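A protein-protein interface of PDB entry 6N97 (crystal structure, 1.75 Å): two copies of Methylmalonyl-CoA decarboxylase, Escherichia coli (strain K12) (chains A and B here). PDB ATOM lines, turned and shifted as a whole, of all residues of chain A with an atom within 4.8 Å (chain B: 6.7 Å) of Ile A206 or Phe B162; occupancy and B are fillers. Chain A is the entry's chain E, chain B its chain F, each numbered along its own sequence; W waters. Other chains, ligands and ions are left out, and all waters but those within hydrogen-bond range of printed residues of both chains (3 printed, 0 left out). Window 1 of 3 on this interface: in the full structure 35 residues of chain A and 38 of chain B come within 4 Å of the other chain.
Of the 12 printed residues of chain B, 7 touch a printed residue of chain A. Along chain B the printed residues that touch a printed residue of chain A span positions 134 to 163. Of the 14 printed residues of chain A, 10 touch a printed residue of chain B. Hydrophobic or aromatic side chains of chain A within 4 Å of the printed part of chain B: Pro A98, Leu A120, Ile A198, Ala A202, Ala A205, Ile A206 and Ile A209. Among the printed residues, 15 pairs touch across the chains.
Pro A98 touches Phe B162 (CG to CD2, 3.7 Å). Leu A120 touches Glu B159. Ile A198 touches Phe B162. Ile A198 touches Thr B163. Lys A201 touches Val B134. Phe B162 touches Lys A201 (O to CG, 3.7 Å). O of Thr B163 touches CE of Lys A201, 3.4 Å away. Val B138 touches Ala A205 (O to CB, 3.5 Å). Ile A206 touches Phe B162. CB of Lys A210 touches CZ of Phe B162, 3.8 Å away.
No position is printed for both chains. Of the 15 pairs that touch across the chains among the printed residues, none has its exchanged pair printed and touching as well.
Of the printed residues of chain B, Ile A198 touches Phe B162 and Thr B163. Of the printed residues of chain B, Ala A202 touches Val B134 (2.9 Å). Of chain B, only Val B134 and Phe B162 come within 4 Å of Ile A206. Printed residues of chain A within 4 Å of Glu B159: Leu A120.
Water W3 lies within hydrogen-bond range of the side-chain carboxylate of Asp A119 (2.6 Å) and the side-chain amino group of Lys B158 (3.3 Å). Water W2 lies within hydrogen-bond range of NZ of Lys B158 (2.7 Å) and O of Lys A210 (3.0 Å). Water W1 lies within hydrogen-bond range of the side-chain amino group of Lys A201 (2.9 Å), the backbone carbonyl oxygen of Thr B163 (3.0 Å) and the backbone carbonyl oxygen of Ala B164 (3.2 Å).
O of Glu B159 lies within hydrogen-bond range of OG1 of Thr B163 (2.7 Å). The backbone NH (N) of Ser B165 lies close to the side-chain hydroxyl (OG1) of Thr B163, at 3.1 Å. OD2 of Asp A119 lies within salt-bridge range of NZ of Lys A210.
O of Val B134 sits at hydrogen-bond distance from N of Ala A202 (2.9 Å). The side-chain carboxylate (OD1) of Asp A119 is in salt-bridge range of the side-chain amino group (NZ) of Lys B158 (2.9 Å).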
ATOM      1  N   PRO A  98     -27.758 -18.533 -30.334  1.00  0.00           N
ATOM      2  CA  PRO A  98     -27.507 -17.139 -29.993  1.00  0.00           C
ATOM      3  C   PRO A  98     -27.709 -16.246 -31.214  1.00  0.00           C
ATOM      4  O   PRO A  98     -27.283 -16.605 -32.321  1.00  0.00           O
ATOM      5  CB  PRO A  98     -26.063 -17.133 -29.504  1.00  0.00           C
ATOM      6  CG  PRO A  98     -25.816 -18.563 -29.094  1.00  0.00           C
ATOM      7  CD  PRO A  98     -26.561 -19.368 -30.116  1.00  0.00           C
ATOM      8  N   ASP A 119     -29.565 -11.715 -27.940  1.00  0.00           N
ATOM      9  CA  ASP A 119     -28.766 -12.286 -26.824  1.00  0.00           C
ATOM     10  C   ASP A 119     -27.558 -11.412 -26.443  1.00  0.00           C
ATOM     11  O   ASP A 119     -27.255 -11.354 -25.217  1.00  0.00           O
ATOM     12  CB  ASP A 119     -28.385 -13.709 -27.200  1.00  0.00           C
ATOM     13  CG  ASP A 119     -29.608 -14.550 -27.488  1.00  0.00           C
ATOM     14  OD1 ASP A 119     -30.531 -14.557 -26.595  1.00  0.00           O
ATOM     15  OD2 ASP A 119     -29.683 -15.139 -28.586  1.00  0.00           O
ATOM     16  N   LEU A 120     -26.869 -10.814 -27.430  1.00  0.00           N
ATOM     17  CA  LEU A 120     -25.678  -9.958 -27.233  1.00  0.00           C
ATOM     18  C   LEU A 120     -25.832  -8.755 -28.172  1.00  0.00           C
ATOM     19  O   LEU A 120     -26.428  -8.903 -29.251  1.00  0.00           O
ATOM     20  CB  LEU A 120     -24.367 -10.661 -27.570  1.00  0.00           C
ATOM     21  CG  LEU A 120     -23.791 -11.642 -26.568  1.00  0.00           C
ATOM     22  CD1 LEU A 120     -24.557 -12.941 -26.608  1.00  0.00           C
ATOM     23  CD2 LEU A 120     -22.322 -11.912 -26.883  1.00  0.00           C
ATOM     24  N   ILE A 198     -18.203 -18.931 -30.028  1.00  0.00           N
ATOM     25  CA  ILE A 198     -19.458 -19.503 -29.465  1.00  0.00           C
ATOM     26  C   ILE A 198     -19.806 -20.767 -30.241  1.00  0.00           C
ATOM     27  O   ILE A 198     -20.187 -21.781 -29.611  1.00  0.00           O
ATOM     28  CB  ILE A 198     -20.584 -18.455 -29.506  1.00  0.00           C
ATOM     29  CG1 ILE A 198     -20.294 -17.280 -28.567  1.00  0.00           C
ATOM     30  CG2 ILE A 198     -21.923 -19.106 -29.255  1.00  0.00           C
ATOM     31  CD1 ILE A 198     -21.269 -16.114 -28.692  1.00  0.00           C
ATOM     32  N   LYS A 201     -18.814 -24.278 -29.132  1.00  0.00           N
ATOM     33  CA  LYS A 201     -19.358 -24.740 -27.838  1.00  0.00           C
ATOM     34  C   LYS A 201     -20.573 -25.643 -28.110  1.00  0.00           C
ATOM     35  O   LYS A 201     -21.069 -25.765 -29.251  1.00  0.00           O
ATOM     36  CB  LYS A 201     -19.655 -23.507 -26.955  1.00  0.00           C
ATOM     37  CG  LYS A 201     -18.505 -22.526 -26.751  1.00  0.00           C
ATOM     38  CD  LYS A 201     -17.232 -23.150 -26.140  1.00  0.00           C
ATOM     39  CE  LYS A 201     -16.109 -22.163 -25.931  1.00  0.00           C
ATOM     40  NZ  LYS A 201     -14.956 -22.777 -25.232  1.00  0.00           N
ATOM     41  N   ALA A 202     -21.098 -26.218 -27.061  1.00  0.00           N
ATOM     42  CA  ALA A 202     -22.147 -27.229 -27.131  1.00  0.00           C
ATOM     43  C   ALA A 202     -23.480 -26.579 -27.437  1.00  0.00           C
ATOM     44  O   ALA A 202     -24.045 -25.910 -26.596  1.00  0.00           O
ATOM     45  CB  ALA A 202     -22.186 -27.997 -25.834  1.00  0.00           C
ATOM     46  N   PRO A 203     -24.042 -26.818 -28.636  1.00  0.00           N
ATOM     47  CA  PRO A 203     -25.252 -26.119 -29.047  1.00  0.00           C
ATOM     48  C   PRO A 203     -26.509 -26.510 -28.266  1.00  0.00           C
ATOM     49  O   PRO A 203     -27.369 -25.686 -28.082  1.00  0.00           O
ATOM     50  CB  PRO A 203     -25.356 -26.477 -30.540  1.00  0.00           C
ATOM     51  CG  PRO A 203     -24.645 -27.820 -30.645  1.00  0.00           C
ATOM     52  CD  PRO A 203     -23.490 -27.700 -29.680  1.00  0.00           C
ATOM     53  N   LEU A 204     -26.607 -27.747 -27.785  1.00  0.00           N
ATOM     54  CA  LEU A 204     -27.820 -28.158 -27.062  1.00  0.00           C
ATOM     55  C   LEU A 204     -27.763 -27.536 -25.665  1.00  0.00           C
ATOM     56  O   LEU A 204     -28.832 -27.203 -25.120  1.00  0.00           O
ATOM     57  CB  LEU A 204     -27.875 -29.685 -27.012  1.00  0.00           C
ATOM     58  CG  LEU A 204     -27.892 -30.404 -28.361  1.00  0.00           C
ATOM     59  CD1 LEU A 204     -27.804 -31.908 -28.102  1.00  0.00           C
ATOM     60  CD2 LEU A 204     -29.135 -30.034 -29.142  1.00  0.00           C
ATOM     61  N   ALA A 205     -26.564 -27.363 -25.095  1.00  0.00           N
ATOM     62  CA  ALA A 205     -26.430 -26.687 -23.784  1.00  0.00           C
ATOM     63  C   ALA A 205     -26.763 -25.190 -23.958  1.00  0.00           C
ATOM     64  O   ALA A 205     -27.532 -24.640 -23.150  1.00  0.00           O
ATOM     65  CB  ALA A 205     -25.044 -26.894 -23.208  1.00  0.00           C
ATOM     66  N   ILE A 206     -26.224 -24.545 -24.985  1.00  0.00           N
ATOM     67  CA  ILE A 206     -26.561 -23.125 -25.307  1.00  0.00           C
ATOM     68  C   ILE A 206     -28.084 -23.013 -25.438  1.00  0.00           C
ATOM     69  O   ILE A 206     -28.673 -22.114 -24.816  1.00  0.00           O
ATOM     70  CB  ILE A 206     -25.803 -22.647 -26.561  1.00  0.00           C
ATOM     71  CG1 ILE A 206     -24.309 -22.452 -26.239  1.00  0.00           C
ATOM     72  CG2 ILE A 206     -26.412 -21.387 -27.117  1.00  0.00           C
ATOM     73  CD1 ILE A 206     -23.448 -22.385 -27.479  1.00  0.00           C
ATOM     74  N   ALA A 207     -28.706 -23.884 -26.229  1.00  0.00           N
ATOM     75  CA  ALA A 207     -30.149 -23.744 -26.521  1.00  0.00           C
ATOM     76  C   ALA A 207     -30.949 -23.872 -25.228  1.00  0.00           C
ATOM     77  O   ALA A 207     -31.892 -23.108 -25.033  1.00  0.00           O
ATOM     78  CB  ALA A 207     -30.604 -24.748 -27.539  1.00  0.00           C
ATOM     79  N   VAL A 208     -30.644 -24.849 -24.375  1.00  0.00           N
ATOM     80  CA  VAL A 208     -31.505 -25.053 -23.172  1.00  0.00           C
ATOM     81  C   VAL A 208     -31.247 -23.903 -22.189  1.00  0.00           C
ATOM     82  O   VAL A 208     -32.207 -23.420 -21.572  1.00  0.00           O
ATOM     83  CB  VAL A 208     -31.427 -26.455 -22.553  1.00  0.00           C
ATOM     84  CG1 VAL A 208     -30.109 -26.738 -21.883  1.00  0.00           C
ATOM     85  CG2 VAL A 208     -32.573 -26.688 -21.575  1.00  0.00           C
ATOM     86  N   ILE A 209     -30.025 -23.417 -22.078  1.00  0.00           N
ATOM     87  CA  ILE A 209     -29.744 -22.309 -21.155  1.00  0.00           C
ATOM     88  C   ILE A 209     -30.387 -21.032 -21.690  1.00  0.00           C
ATOM     89  O   ILE A 209     -30.990 -20.297 -20.887  1.00  0.00           O
ATOM     90  CB  ILE A 209     -28.245 -22.161 -20.891  1.00  0.00           C
ATOM     91  CG1 ILE A 209     -27.724 -23.388 -20.142  1.00  0.00           C
ATOM     92  CG2 ILE A 209     -28.011 -20.844 -20.153  1.00  0.00           C
ATOM     93  CD1 ILE A 209     -26.177 -23.571 -20.125  1.00  0.00           C
ATOM     94  N   LYS A 210     -30.338 -20.795 -22.998  1.00  0.00           N
ATOM     95  CA  LYS A 210     -31.058 -19.635 -23.580  1.00  0.00           C
ATOM     96  C   LYS A 210     -32.534 -19.723 -23.215  1.00  0.00           C
ATOM     97  O   LYS A 210     -33.158 -18.666 -22.876  1.00  0.00           O
ATOM     98  CB  LYS A 210     -30.890 -19.565 -25.093  1.00  0.00           C
ATOM     99  CG  LYS A 210     -31.648 -18.412 -25.701  1.00  0.00           C
ATOM    100  CD  LYS A 210     -31.290 -18.161 -27.127  1.00  0.00           C
ATOM    101  CE  LYS A 210     -32.290 -17.207 -27.745  1.00  0.00           C
ATOM    102  NZ  LYS A 210     -31.862 -16.722 -29.060  1.00  0.00           N
ATOM    103  N   MET B 131     -17.904 -19.076 -16.551  1.00  0.00           N
ATOM    104  CA  MET B 131     -19.060 -19.982 -16.392  1.00  0.00           C
ATOM    105  C   MET B 131     -18.997 -20.933 -17.577  1.00  0.00           C
ATOM    106  O   MET B 131     -19.067 -20.444 -18.697  1.00  0.00           O
ATOM    107  CB  MET B 131     -20.374 -19.191 -16.318  1.00  0.00           C
ATOM    108  CG  MET B 131     -21.515 -20.029 -15.781  1.00  0.00           C
ATOM    109  SD  MET B 131     -21.161 -20.672 -14.186  1.00  0.00           S
ATOM    110  CE  MET B 131     -22.331 -22.018 -14.002  1.00  0.00           C
ATOM    111  N   VAL B 134     -21.204 -24.799 -21.308  1.00  0.00           N
ATOM    112  CA  VAL B 134     -21.221 -25.018 -22.782  1.00  0.00           C
ATOM    113  C   VAL B 134     -19.867 -25.600 -23.255  1.00  0.00           C
ATOM    114  O   VAL B 134     -19.818 -26.054 -24.409  1.00  0.00           O
ATOM    115  CB  VAL B 134     -21.583 -23.734 -23.541  1.00  0.00           C
ATOM    116  CG1 VAL B 134     -22.851 -23.150 -23.019  1.00  0.00           C
ATOM    117  CG2 VAL B 134     -20.490 -22.707 -23.540  1.00  0.00           C
ATOM    118  N   VAL B 138     -23.169 -29.471 -20.687  1.00  0.00           N
ATOM    119  CA  VAL B 138     -24.036 -29.621 -19.475  1.00  0.00           C
ATOM    120  C   VAL B 138     -25.311 -28.810 -19.601  1.00  0.00           C
ATOM    121  O   VAL B 138     -25.209 -27.593 -19.764  1.00  0.00           O
ATOM    122  CB  VAL B 138     -23.274 -29.159 -18.230  1.00  0.00           C
ATOM    123  CG1 VAL B 138     -24.167 -29.118 -17.018  1.00  0.00           C
ATOM    124  CG2 VAL B 138     -22.072 -30.039 -17.994  1.00  0.00           C
ATOM    125  N   VAL B 157     -24.812 -11.801 -18.953  1.00  0.00           N
ATOM    126  CA  VAL B 157     -24.842 -13.198 -18.478  1.00  0.00           C
ATOM    127  C   VAL B 157     -24.781 -14.102 -19.719  1.00  0.00           C
ATOM    128  O   VAL B 157     -24.062 -15.117 -19.712  1.00  0.00           O
ATOM    129  CB  VAL B 157     -26.092 -13.449 -17.630  1.00  0.00           C
ATOM    130  CG1 VAL B 157     -26.341 -14.919 -17.404  1.00  0.00           C
ATOM    131  CG2 VAL B 157     -25.996 -12.664 -16.338  1.00  0.00           C
ATOM    132  N   LYS B 158     -25.548 -13.795 -20.772  1.00  0.00           N
ATOM    133  CA  LYS B 158     -25.506 -14.631 -22.007  1.00  0.00           C
ATOM    134  C   LYS B 158     -24.117 -14.635 -22.642  1.00  0.00           C
ATOM    135  O   LYS B 158     -23.665 -15.720 -23.059  1.00  0.00           O
ATOM    136  CB  LYS B 158     -26.582 -14.191 -22.996  1.00  0.00           C
ATOM    137  CG  LYS B 158     -27.950 -14.594 -22.496  1.00  0.00           C
ATOM    138  CD  LYS B 158     -28.986 -13.814 -23.262  1.00  0.00           C
ATOM    139  CE  LYS B 158     -30.391 -14.189 -22.961  1.00  0.00           C
ATOM    140  NZ  LYS B 158     -31.270 -13.614 -23.995  1.00  0.00           N
ATOM    141  N   GLU B 159     -23.417 -13.502 -22.659  1.00  0.00           N
ATOM    142  CA  GLU B 159     -22.002 -13.526 -23.128  1.00  0.00           C
ATOM    143  C   GLU B 159     -21.172 -14.482 -22.275  1.00  0.00           C
ATOM    144  O   GLU B 159     -20.433 -15.301 -22.847  1.00  0.00           O
ATOM    145  CB  GLU B 159     -21.424 -12.121 -23.204  1.00  0.00           C
ATOM    146  CG  GLU B 159     -19.941 -12.125 -23.582  1.00  0.00           C
ATOM    147  CD  GLU B 159     -19.294 -10.755 -23.549  1.00  0.00           C
ATOM    148  OE1 GLU B 159     -20.007  -9.755 -23.312  1.00  0.00           O
ATOM    149  OE2 GLU B 159     -18.036 -10.725 -23.623  1.00  0.00           O
ATOM    150  N   LEU B 160     -21.237 -14.351 -20.949  1.00  0.00           N
ATOM    151  CA  LEU B 160     -20.392 -15.162 -20.058  1.00  0.00           C
ATOM    152  C   LEU B 160     -20.655 -16.640 -20.314  1.00  0.00           C
ATOM    153  O   LEU B 160     -19.724 -17.427 -20.438  1.00  0.00           O
ATOM    154  CB  LEU B 160     -20.770 -14.858 -18.603  1.00  0.00           C
ATOM    155  CG  LEU B 160     -20.063 -13.715 -17.916  1.00  0.00           C
ATOM    156  CD1 LEU B 160     -20.572 -13.656 -16.477  1.00  0.00           C
ATOM    157  CD2 LEU B 160     -18.552 -13.925 -17.921  1.00  0.00           C
ATOM    158  N   ILE B 161     -21.928 -17.011 -20.422  1.00  0.00           N
ATOM    159  CA  ILE B 161     -22.293 -18.433 -20.578  1.00  0.00           C
ATOM    160  C   ILE B 161     -22.059 -18.897 -22.014  1.00  0.00           C
ATOM    161  O   ILE B 161     -21.502 -20.043 -22.171  1.00  0.00           O
ATOM    162  CB  ILE B 161     -23.740 -18.636 -20.149  1.00  0.00           C
ATOM    163  CG1 ILE B 161     -23.881 -18.313 -18.674  1.00  0.00           C
ATOM    164  CG2 ILE B 161     -24.219 -20.038 -20.476  1.00  0.00           C
ATOM    165  CD1 ILE B 161     -25.349 -18.311 -18.230  1.00  0.00           C
ATOM    166  N   PHE B 162     -22.447 -18.122 -23.026  1.00  0.00           N
ATOM    167  CA  PHE B 162     -22.360 -18.657 -24.424  1.00  0.00           C
ATOM    168  C   PHE B 162     -20.894 -18.740 -24.873  1.00  0.00           C
ATOM    169  O   PHE B 162     -20.542 -19.642 -25.624  1.00  0.00           O
ATOM    170  CB  PHE B 162     -23.206 -17.868 -25.397  1.00  0.00           C
ATOM    171  CG  PHE B 162     -24.700 -17.896 -25.130  1.00  0.00           C
ATOM    172  CD1 PHE B 162     -25.274 -18.819 -24.274  1.00  0.00           C
ATOM    173  CD2 PHE B 162     -25.511 -16.971 -25.747  1.00  0.00           C
ATOM    174  CE1 PHE B 162     -26.651 -18.834 -24.072  1.00  0.00           C
ATOM    175  CE2 PHE B 162     -26.880 -16.979 -25.531  1.00  0.00           C
ATOM    176  CZ  PHE B 162     -27.447 -17.912 -24.709  1.00  0.00           C
ATOM    177  N   THR B 163     -20.034 -17.867 -24.385  1.00  0.00           N
ATOM    178  CA  THR B 163     -18.598 -17.886 -24.755  1.00  0.00           C
ATOM    179  C   THR B 163     -17.809 -18.795 -23.823  1.00  0.00           C
ATOM    180  O   THR B 163     -16.758 -19.262 -24.238  1.00  0.00           O
ATOM    181  CB  THR B 163     -17.961 -16.490 -24.762  1.00  0.00           C
ATOM    182  OG1 THR B 163     -17.876 -15.975 -23.430  1.00  0.00           O
ATOM    183  CG2 THR B 163     -18.717 -15.500 -25.614  1.00  0.00           C
ATOM    184  N   ALA B 164     -18.227 -18.960 -22.582  1.00  0.00           N
ATOM    185  CA  ALA B 164     -17.424 -19.607 -21.518  1.00  0.00           C
ATOM    186  C   ALA B 164     -16.058 -18.936 -21.390  1.00  0.00           C
ATOM    187  O   ALA B 164     -15.139 -19.605 -20.874  1.00  0.00           O
ATOM    188  CB  ALA B 164     -17.268 -21.092 -21.777  1.00  0.00           C
ATOM    189  N   SER B 165     -15.904 -17.676 -21.800  1.00  0.00           N
ATOM    190  CA  SER B 165     -14.569 -17.012 -21.740  1.00  0.00           C
ATOM    191  C   SER B 165     -14.424 -16.380 -20.365  1.00  0.00           C
ATOM    192  O   SER B 165     -15.386 -15.852 -19.802  1.00  0.00           O
ATOM    193  CB  SER B 165     -14.428 -15.948 -22.804  1.00  0.00           C
ATOM    194  OG  SER B 165     -14.543 -16.498 -24.090  1.00  0.00           O
HETATM  195  O   HOH W   1     -13.997 -20.414 -23.804  1.00  0.00           O
HETATM  196  O   HOH W   2     -32.895 -15.645 -23.185  1.00  0.00           O
HETATM  197  O   HOH W   3     -32.927 -13.698 -26.833  1.00  0.00           O
